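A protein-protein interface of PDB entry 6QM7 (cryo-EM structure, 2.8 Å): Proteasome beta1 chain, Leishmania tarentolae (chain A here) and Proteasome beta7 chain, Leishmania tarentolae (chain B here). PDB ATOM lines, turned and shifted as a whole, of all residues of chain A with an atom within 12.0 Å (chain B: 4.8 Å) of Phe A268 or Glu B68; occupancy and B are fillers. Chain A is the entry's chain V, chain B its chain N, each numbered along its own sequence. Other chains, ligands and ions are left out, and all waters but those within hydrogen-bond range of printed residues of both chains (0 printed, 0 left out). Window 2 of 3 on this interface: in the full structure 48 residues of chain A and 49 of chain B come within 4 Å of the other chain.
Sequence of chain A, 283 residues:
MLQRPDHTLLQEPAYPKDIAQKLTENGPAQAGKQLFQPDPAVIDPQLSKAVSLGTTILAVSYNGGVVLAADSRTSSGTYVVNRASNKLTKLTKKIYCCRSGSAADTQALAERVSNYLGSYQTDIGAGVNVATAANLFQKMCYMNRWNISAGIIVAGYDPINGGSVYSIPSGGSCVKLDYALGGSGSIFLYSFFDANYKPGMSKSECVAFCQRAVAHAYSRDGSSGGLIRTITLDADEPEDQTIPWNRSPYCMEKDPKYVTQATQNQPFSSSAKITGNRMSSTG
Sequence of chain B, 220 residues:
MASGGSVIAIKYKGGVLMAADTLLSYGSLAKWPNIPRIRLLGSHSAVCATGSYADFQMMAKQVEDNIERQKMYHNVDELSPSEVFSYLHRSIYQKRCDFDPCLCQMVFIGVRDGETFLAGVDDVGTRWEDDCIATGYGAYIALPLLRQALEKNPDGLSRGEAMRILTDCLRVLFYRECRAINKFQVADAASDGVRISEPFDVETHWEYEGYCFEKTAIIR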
ATOM      1  N   THR A 263      11.598 -19.432  12.701  1.00  0.00           N
ATOM      2  CA  THR A 263      12.292 -18.979  11.478  1.00  0.00           C
ATOM      3  C   THR A 263      12.362 -17.457  11.544  1.00  0.00           C
ATOM      4  O   THR A 263      11.549 -16.792  10.910  1.00  0.00           O
ATOM      5  CB  THR A 263      11.626 -19.549  10.228  1.00  0.00           C
ATOM      6  OG1 THR A 263      11.553 -20.967  10.371  1.00  0.00           O
ATOM      7  CG2 THR A 263      12.409 -19.209   8.982  1.00  0.00           C
ATOM      8  N   GLN A 264      13.286 -16.949  12.347  1.00  0.00           N
ATOM      9  CA  GLN A 264      13.448 -15.506  12.629  1.00  0.00           C
ATOM     10  C   GLN A 264      14.526 -14.910  11.737  1.00  0.00           C
ATOM     11  O   GLN A 264      14.430 -13.700  11.455  1.00  0.00           O
ATOM     12  CB  GLN A 264      13.872 -15.293  14.080  1.00  0.00           C
ATOM     13  CG  GLN A 264      12.741 -15.518  15.064  1.00  0.00           C
ATOM     14  CD  GLN A 264      11.575 -14.616  14.749  1.00  0.00           C
ATOM     15  OE1 GLN A 264      10.667 -14.983  14.008  1.00  0.00           O
ATOM     16  NE2 GLN A 264      11.631 -13.403  15.264  1.00  0.00           N
ATOM     17  N   ASN A 265      15.544 -15.701  11.380  1.00  0.00           N
ATOM     18  CA  ASN A 265      16.805 -15.159  10.824  1.00  0.00           C
ATOM     19  C   ASN A 265      16.622 -15.067   9.316  1.00  0.00           C
ATOM     20  O   ASN A 265      16.377 -13.934   8.848  1.00  0.00           O
ATOM     21  CB  ASN A 265      18.012 -15.914  11.355  1.00  0.00           C
ATOM     22  CG  ASN A 265      18.264 -15.599  12.819  1.00  0.00           C
ATOM     23  OD1 ASN A 265      17.827 -14.567  13.335  1.00  0.00           O
ATOM     24  ND2 ASN A 265      18.987 -16.479  13.496  1.00  0.00           N
ATOM     25  N   GLN A 266      16.663 -16.180   8.602  1.00  0.00           N
ATOM     26  CA  GLN A 266      16.136 -16.269   7.212  1.00  0.00           C
ATOM     27  C   GLN A 266      17.140 -15.673   6.243  1.00  0.00           C
ATOM     28  O   GLN A 266      17.455 -14.490   6.325  1.00  0.00           O
ATOM     29  CB  GLN A 266      14.794 -15.554   7.062  1.00  0.00           C
ATOM     30  CG  GLN A 266      13.856 -16.205   6.061  1.00  0.00           C
ATOM     31  CD  GLN A 266      12.468 -15.641   6.252  1.00  0.00           C
ATOM     32  OE1 GLN A 266      11.918 -14.978   5.374  1.00  0.00           O
ATOM     33  NE2 GLN A 266      11.906 -15.862   7.431  1.00  0.00           N
ATOM     34  N   PRO A 267      17.664 -16.472   5.291  1.00  0.00           N
ATOM     35  CA  PRO A 267      18.666 -15.975   4.364  1.00  0.00           C
ATOM     36  C   PRO A 267      18.004 -14.983   3.413  1.00  0.00           C
ATOM     37  O   PRO A 267      16.807 -15.065   3.196  1.00  0.00           O
ATOM     38  CB  PRO A 267      19.185 -17.209   3.622  1.00  0.00           C
ATOM     39  CG  PRO A 267      18.082 -18.240   3.784  1.00  0.00           C
ATOM     40  CD  PRO A 267      17.333 -17.881   5.051  1.00  0.00           C
ATOM     41  N   PHE A 268      18.817 -14.077   2.890  1.00  0.00           N
ATOM     42  CA  PHE A 268      18.459 -13.133   1.810  1.00  0.00           C
ATOM     43  C   PHE A 268      18.154 -13.942   0.546  1.00  0.00           C
ATOM     44  O   PHE A 268      19.085 -14.591   0.002  1.00  0.00           O
ATOM     45  CB  PHE A 268      19.612 -12.157   1.612  1.00  0.00           C
ATOM     46  CG  PHE A 268      19.296 -11.009   0.699  1.00  0.00           C
ATOM     47  CD1 PHE A 268      20.085 -10.759  -0.415  1.00  0.00           C
ATOM     48  CD2 PHE A 268      18.222 -10.174   0.964  1.00  0.00           C
ATOM     49  CE1 PHE A 268      19.812  -9.687  -1.242  1.00  0.00           C
ATOM     50  CE2 PHE A 268      17.947  -9.104   0.132  1.00  0.00           C
ATOM     51  CZ  PHE A 268      18.742  -8.862  -0.969  1.00  0.00           C
ATOM     52  N   SER A 269      16.885 -13.946   0.126  1.00  0.00           N
ATOM     53  CA  SER A 269      16.373 -14.839  -0.942  1.00  0.00           C
ATOM     54  C   SER A 269      15.703 -14.029  -2.044  1.00  0.00           C
ATOM     55  O   SER A 269      15.481 -12.844  -1.862  1.00  0.00           O
ATOM     56  CB  SER A 269      15.433 -15.862  -0.385  1.00  0.00           C
ATOM     57  OG  SER A 269      14.153 -15.300  -0.204  1.00  0.00           O
ATOM     58  N   SER A 270      15.410 -14.686  -3.157  1.00  0.00           N
ATOM     59  CA  SER A 270      14.759 -14.096  -4.348  1.00  0.00           C
ATOM     60  C   SER A 270      13.286 -14.497  -4.349  1.00  0.00           C
ATOM     61  O   SER A 270      12.644 -14.396  -5.399  1.00  0.00           O
ATOM     62  CB  SER A 270      15.468 -14.566  -5.579  1.00  0.00           C
ATOM     63  OG  SER A 270      16.830 -14.164  -5.564  1.00  0.00           O
ATOM     64  N   SER A 271      12.791 -14.939  -3.195  1.00  0.00           N
ATOM     65  CA  SER A 271      11.467 -15.577  -3.011  1.00  0.00           C
ATOM     66  C   SER A 271      10.937 -15.204  -1.627  1.00  0.00           C
ATOM     67  O   SER A 271      11.752 -15.043  -0.718  1.00  0.00           O
ATOM     68  CB  SER A 271      11.568 -17.074  -3.177  1.00  0.00           C
ATOM     69  OG  SER A 271      10.276 -17.669  -3.184  1.00  0.00           O
ATOM     70  N   ALA A 272       9.619 -15.068  -1.487  1.00  0.00           N
ATOM     71  CA  ALA A 272       8.925 -14.827  -0.200  1.00  0.00           C
ATOM     72  C   ALA A 272       8.716 -16.156   0.535  1.00  0.00           C
ATOM     73  O   ALA A 272       8.201 -16.118   1.673  1.00  0.00           O
ATOM     74  CB  ALA A 272       7.613 -14.134  -0.457  1.00  0.00           C
ATOM     75  N   LYS A 273       9.071 -17.282  -0.095  1.00  0.00           N
ATOM     76  CA  LYS A 273       9.038 -18.616   0.540  1.00  0.00           C
ATOM     77  C   LYS A 273       9.993 -18.626   1.735  1.00  0.00           C
ATOM     78  O   LYS A 273      11.203 -18.513   1.514  1.00  0.00           O
ATOM     79  CB  LYS A 273       9.410 -19.724  -0.446  1.00  0.00           C
ATOM     80  CG  LYS A 273       9.358 -21.116   0.174  1.00  0.00           C
ATOM     81  CD  LYS A 273       8.836 -22.211  -0.747  1.00  0.00           C
ATOM     82  CE  LYS A 273       7.710 -23.023  -0.136  1.00  0.00           C
ATOM     83  NZ  LYS A 273       8.055 -23.547   1.209  1.00  0.00           N
ATOM     84  N   ILE A 274       9.448 -18.734   2.950  1.00  0.00           N
ATOM     85  CA  ILE A 274      10.211 -18.990   4.205  1.00  0.00           C
ATOM     86  C   ILE A 274      10.722 -20.429   4.124  1.00  0.00           C
ATOM     87  O   ILE A 274       9.881 -21.337   4.009  1.00  0.00           O
ATOM     88  CB  ILE A 274       9.351 -18.729   5.466  1.00  0.00           C
ATOM     89  CG1 ILE A 274       9.263 -17.236   5.810  1.00  0.00           C
ATOM     90  CG2 ILE A 274       9.858 -19.533   6.657  1.00  0.00           C
ATOM     91  CD1 ILE A 274       8.038 -16.529   5.284  1.00  0.00           C
ATOM     92  N   THR A 275      12.048 -20.608   4.176  1.00  0.00           N
ATOM     93  CA  THR A 275      12.748 -21.921   4.144  1.00  0.00           C
ATOM     94  C   THR A 275      13.125 -22.326   5.576  1.00  0.00           C
ATOM     95  O   THR A 275      12.442 -23.195   6.159  1.00  0.00           O
ATOM     96  CB  THR A 275      13.969 -21.871   3.213  1.00  0.00           C
ATOM     97  OG1 THR A 275      14.752 -20.731   3.577  1.00  0.00           O
ATOM     98  CG2 THR A 275      13.598 -21.793   1.746  1.00  0.00           C
ATOM     99  N   GLY A 276      14.167 -21.710   6.120  1.00  0.00           N
ATOM    100  CA  GLY A 276      14.623 -21.922   7.505  1.00  0.00           C
ATOM    101  C   GLY A 276      15.489 -20.766   7.968  1.00  0.00           C
ATOM    102  O   GLY A 276      15.550 -19.753   7.263  1.00  0.00           O
ATOM    103  N   ASN A 277      16.133 -20.904   9.118  1.00  0.00           N
ATOM    104  CA  ASN A 277      17.152 -19.927   9.559  1.00  0.00           C
ATOM    105  C   ASN A 277      18.405 -20.139   8.712  1.00  0.00           C
ATOM    106  O   ASN A 277      18.677 -21.286   8.304  1.00  0.00           O
ATOM    107  CB  ASN A 277      17.447 -20.025  11.053  1.00  0.00           C
ATOM    108  CG  ASN A 277      16.213 -19.716  11.860  1.00  0.00           C
ATOM    109  OD1 ASN A 277      15.665 -18.624  11.753  1.00  0.00           O
ATOM    110  ND2 ASN A 277      15.759 -20.671  12.652  1.00  0.00           N
ATOM    111  N   ARG A 278      19.117 -19.046   8.460  1.00  0.00           N
ATOM    112  CA  ARG A 278      20.491 -19.028   7.918  1.00  0.00           C
ATOM    113  C   ARG A 278      21.423 -19.428   9.060  1.00  0.00           C
ATOM    114  O   ARG A 278      21.383 -18.750  10.124  1.00  0.00           O
ATOM    115  CB  ARG A 278      20.790 -17.624   7.393  1.00  0.00           C
ATOM    116  CG  ARG A 278      22.088 -17.499   6.621  1.00  0.00           C
ATOM    117  CD  ARG A 278      22.375 -16.044   6.359  1.00  0.00           C
ATOM    118  NE  ARG A 278      23.687 -15.913   5.745  1.00  0.00           N
ATOM    119  CZ  ARG A 278      24.428 -14.808   5.746  1.00  0.00           C
ATOM    120  NH1 ARG A 278      25.607 -14.826   5.146  1.00  0.00           N
ATOM    121  NH2 ARG A 278      23.997 -13.688   6.318  1.00  0.00           N
ATOM    122  N   MET A 279      22.191 -20.503   8.860  1.00  0.00           N
ATOM    123  CA  MET A 279      23.015 -21.145   9.919  1.00  0.00           C
ATOM    124  C   MET A 279      24.469 -21.317   9.479  1.00  0.00           C
ATOM    125  O   MET A 279      25.236 -21.900  10.247  1.00  0.00           O
ATOM    126  CB  MET A 279      22.374 -22.481  10.297  1.00  0.00           C
ATOM    127  CG  MET A 279      21.028 -22.238  10.966  1.00  0.00           C
ATOM    128  SD  MET A 279      20.450 -23.545  12.047  1.00  0.00           S
ATOM    129  CE  MET A 279      21.698 -23.548  13.332  1.00  0.00           C
ATOM    130  N   SER A 280      24.835 -20.755   8.330  1.00  0.00           N
ATOM    131  CA  SER A 280      26.194 -20.791   7.738  1.00  0.00           C
ATOM    132  C   SER A 280      26.326 -19.578   6.829  1.00  0.00           C
ATOM    133  O   SER A 280      25.362 -19.284   6.108  1.00  0.00           O
ATOM    134  CB  SER A 280      26.447 -22.062   6.969  1.00  0.00           C
ATOM    135  OG  SER A 280      26.826 -23.124   7.833  1.00  0.00           O
ATOM    136  N   SER A 281      27.460 -18.898   6.870  1.00  0.00           N
ATOM    137  CA  SER A 281      27.702 -17.677   6.070  1.00  0.00           C
ATOM    138  C   SER A 281      27.776 -18.036   4.584  1.00  0.00           C
ATOM    139  O   SER A 281      27.278 -17.237   3.763  1.00  0.00           O
ATOM    140  CB  SER A 281      28.924 -16.971   6.549  1.00  0.00           C
ATOM    141  OG  SER A 281      28.651 -16.310   7.780  1.00  0.00           O
ATOM    142  N   THR A 282      28.340 -19.211   4.271  1.00  0.00           N
ATOM    143  CA  THR A 282      28.453 -19.807   2.906  1.00  0.00           C
ATOM    144  C   THR A 282      27.064 -20.082   2.295  1.00  0.00           C
ATOM    145  O   THR A 282      26.976 -20.069   1.052  1.00  0.00           O
ATOM    146  CB  THR A 282      29.313 -21.081   2.942  1.00  0.00           C
ATOM    147  OG1 THR A 282      28.713 -22.001   3.855  1.00  0.00           O
ATOM    148  CG2 THR A 282      30.748 -20.819   3.352  1.00  0.00           C
ATOM    149  N   GLY A 283      26.031 -20.329   3.118  1.00  0.00           N
ATOM    150  CA  GLY A 283      24.630 -20.548   2.689  1.00  0.00           C
ATOM    151  C   GLY A 283      23.630 -19.715   3.486  1.00  0.00           C
ATOM    152  O   GLY A 283      22.982 -20.214   4.409  1.00  0.00           O
ATOM    153  OXT GLY A 283      23.415 -18.520   3.246  1.00  0.00           O
ATOM    154  N   GLY B  42      26.051 -10.587   6.815  1.00  0.00           N
ATOM    155  CA  GLY B  42      26.869 -10.826   5.616  1.00  0.00           C
ATOM    156  C   GLY B  42      27.699 -12.081   5.789  1.00  0.00           C
ATOM    157  O   GLY B  42      27.262 -12.988   6.531  1.00  0.00           O
ATOM    158  N   GLU B  64      22.154  -5.586   8.423  1.00  0.00           N
ATOM    159  CA  GLU B  64      22.265  -6.681   7.428  1.00  0.00           C
ATOM    160  C   GLU B  64      21.877  -6.174   6.037  1.00  0.00           C
ATOM    161  O   GLU B  64      22.440  -6.689   5.062  1.00  0.00           O
ATOM    162  CB  GLU B  64      21.410  -7.884   7.828  1.00  0.00           C
ATOM    163  CG  GLU B  64      21.654  -9.108   6.953  1.00  0.00           C
ATOM    164  CD  GLU B  64      21.318 -10.453   7.583  1.00  0.00           C
ATOM    165  OE1 GLU B  64      20.581 -10.467   8.599  1.00  0.00           O
ATOM    166  OE2 GLU B  64      21.798 -11.491   7.052  1.00  0.00           O
ATOM    167  N   ASP B  65      20.947  -5.220   5.956  1.00  0.00           N
ATOM    168  CA  ASP B  65      20.577  -4.529   4.692  1.00  0.00           C
ATOM    169  C   ASP B  65      21.764  -3.708   4.203  1.00  0.00           C
ATOM    170  O   ASP B  65      22.204  -3.934   3.069  1.00  0.00           O
ATOM    171  CB  ASP B  65      19.400  -3.572   4.872  1.00  0.00           C
ATOM    172  CG  ASP B  65      18.055  -4.246   5.100  1.00  0.00           C
ATOM    173  OD1 ASP B  65      17.083  -3.499   5.414  1.00  0.00           O
ATOM    174  OD2 ASP B  65      17.982  -5.508   4.982  1.00  0.00           O
ATOM    175  N   ASN B  66      22.254  -2.805   5.046  1.00  0.00           N
ATOM    176  CA  ASN B  66      23.420  -1.931   4.770  1.00  0.00           C
ATOM    177  C   ASN B  66      24.545  -2.751   4.128  1.00  0.00           C
ATOM    178  O   ASN B  66      25.084  -2.314   3.100  1.00  0.00           O
ATOM    179  CB  ASN B  66      23.916  -1.261   6.049  1.00  0.00           C
ATOM    180  CG  ASN B  66      24.784  -0.059   5.778  1.00  0.00           C
ATOM    181  OD1 ASN B  66      24.277   1.024   5.495  1.00  0.00           O
ATOM    182  ND2 ASN B  66      26.091  -0.250   5.854  1.00  0.00           N
ATOM    183  N   ILE B  67      24.872  -3.904   4.710  1.00  0.00           N
ATOM    184  CA  ILE B  67      25.964  -4.796   4.228  1.00  0.00           C
ATOM    185  C   ILE B  67      25.615  -5.304   2.829  1.00  0.00           C
ATOM    186  O   ILE B  67      26.512  -5.225   1.966  1.00  0.00           O
ATOM    187  CB  ILE B  67      26.210  -5.982   5.175  1.00  0.00           C
ATOM    188  CG1 ILE B  67      26.645  -5.554   6.578  1.00  0.00           C
ATOM    189  CG2 ILE B  67      27.214  -6.947   4.557  1.00  0.00           C
ATOM    190  CD1 ILE B  67      26.546  -6.672   7.618  1.00  0.00           C
ATOM    191  N   GLU B  68      24.413  -5.865   2.632  1.00  0.00           N
ATOM    192  CA  GLU B  68      24.034  -6.549   1.361  1.00  0.00           C
ATOM    193  C   GLU B  68      23.882  -5.513   0.256  1.00  0.00           C
ATOM    194  O   GLU B  68      24.379  -5.765  -0.852  1.00  0.00           O
ATOM    195  CB  GLU B  68      22.749  -7.378   1.461  1.00  0.00           C
ATOM    196  CG  GLU B  68      23.001  -8.880   1.625  1.00  0.00           C
ATOM    197  CD  GLU B  68      22.675  -9.467   2.996  1.00  0.00           C
ATOM    198  OE1 GLU B  68      23.620  -9.828   3.744  1.00  0.00           O
ATOM    199  OE2 GLU B  68      21.466  -9.577   3.310  1.00  0.00           O
ATOM    200  N   ARG B  69      23.217  -4.402   0.566  1.00  0.00           N
ATOM    201  CA  ARG B  69      23.003  -3.263  -0.362  1.00  0.00           C
ATOM    202  C   ARG B  69      24.346  -2.780  -0.915  1.00  0.00           C
ATOM    203  O   ARG B  69      24.530  -2.841  -2.136  1.00  0.00           O
ATOM    204  CB  ARG B  69      22.273  -2.112   0.340  1.00  0.00           C
ATOM    205  CG  ARG B  69      20.814  -1.982  -0.057  1.00  0.00           C
ATOM    206  CD  ARG B  69      19.865  -2.912   0.649  1.00  0.00           C
ATOM    207  NE  ARG B  69      18.948  -2.187   1.525  1.00  0.00           N
ATOM    208  CZ  ARG B  69      17.736  -2.608   1.894  1.00  0.00           C
ATOM    209  NH1 ARG B  69      17.014  -1.845   2.701  1.00  0.00           N
ATOM    210  NH2 ARG B  69      17.244  -3.770   1.469  1.00  0.00           N
ATOM    211  N   GLN B  70      25.246  -2.324  -0.051  1.00  0.00           N
ATOM    212  CA  GLN B  70      26.566  -1.771  -0.454  1.00  0.00           C
ATOM    213  C   GLN B  70      27.259  -2.747  -1.415  1.00  0.00           C
ATOM    214  O   GLN B  70      27.769  -2.288  -2.438  1.00  0.00           O
ATOM    215  CB  GLN B  70      27.435  -1.487   0.773  1.00  0.00           C
ATOM    216  CG  GLN B  70      28.549  -0.483   0.506  1.00  0.00           C
ATOM    217  CD  GLN B  70      29.879  -0.820   1.145  1.00  0.00           C
ATOM    218  OE1 GLN B  70      30.272  -1.984   1.268  1.00  0.00           O
ATOM    219  NE2 GLN B  70      30.610   0.216   1.523  1.00  0.00           N
ATOM    220  N   LYS B  71      27.259  -4.040  -1.093  1.00  0.00           N
ATOM    221  CA  LYS B  71      27.971  -5.113  -1.839  1.00  0.00           C
ATOM    222  C   LYS B  71      27.368  -5.269  -3.231  1.00  0.00           C
ATOM    223  O   LYS B  71      28.123  -5.536  -4.180  1.00  0.00           O
ATOM    224  CB  LYS B  71      27.824  -6.441  -1.093  1.00  0.00           C
ATOM    225  CG  LYS B  71      28.712  -7.594  -1.556  1.00  0.00           C
ATOM    226  CD  LYS B  71      28.190  -8.970  -1.148  1.00  0.00           C
ATOM    227  CE  LYS B  71      27.558  -8.996   0.235  1.00  0.00           C
ATOM    228  NZ  LYS B  71      27.373 -10.374   0.752  1.00  0.00           N
ATOM    229  N   MET B  72      26.045  -5.142  -3.317  1.00  0.00           N
ATOM    230  CA  MET B  72      25.211  -5.487  -4.496  1.00  0.00           C
ATOM    231  C   MET B  72      25.080  -4.280  -5.427  1.00  0.00           C
ATOM    232  O   MET B  72      25.006  -4.479  -6.647  1.00  0.00           O
ATOM    233  CB  MET B  72      23.821  -5.888  -4.004  1.00  0.00           C
ATOM    234  CG  MET B  72      22.843  -6.251  -5.098  1.00  0.00           C
ATOM    235  SD  MET B  72      21.177  -5.951  -4.532  1.00  0.00           S
ATOM    236  CE  MET B  72      21.084  -7.109  -3.169  1.00  0.00           C
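Along chain A the printed residues that touch a printed residue of chain B span positions 268 to 281. Hydrophobic or aromatic side chains of chain B within 4 Å of the printed part of chain A: Met B72. Among the printed residues, 5 pairs touch across the chains.
The guanidinium group (NE) of Arg A278 lies within salt-bridge range of the chain-end carboxylate (OXT) of Gly A283 (3.6 Å). NH1 of Arg A278 is in hydrogen-bond range of O of Ser A281 (3.2 Å).
NH2 of Arg A278 lies within salt-bridge range of OE2 of Glu B64, at 3.2 Å. O of Gly B42 is in hydrogen-bond range of NH1 of Arg A278.
Phe A268 touches just these residues of chain B: Glu B68 (3.6 Å) and Met B72 (3.5 Å). Of chain A, only Phe A268 (3.6 Å) comes within 4 Å of Glu B68. Gly B42 touches two residues of chain A. Printed residues of chain A within 4 Å of Glu B64: Arg A278. No residue of chain A comes within 4 Å of Asp B65. No residue of chain A comes within 4 Å of Asn B66. No residue of chain A comes within 4 Å of Ile B67. Of chain A, only Phe A268 (3.5 Å) comes within 4 Å of Met B72. Of the printed residues of chain B, Arg A278 touches Gly B42 (2.8 Å) and Glu B64 (3.2 Å). Of the printed residues of chain B, Ser A281 touches Gly B42. Ser A269 touches none of the printed residues of chain B. Gly A283 touches none of the printed residues of chain B. The nearest residue of chain A that does not touch Glu B68 is Arg A278 (4.7 Å). The nearest printed residue of chain B that does not touch Arg A278 is Glu B68 (4.7 Å).
OE2 of Glu B68 touches CB of Phe A268 (3.6 Å). Phe A268 touches Met B72 (CE1 to CE, 3.5 Å). OG of Ser A281 touches O of Gly B42 (3.8 Å).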
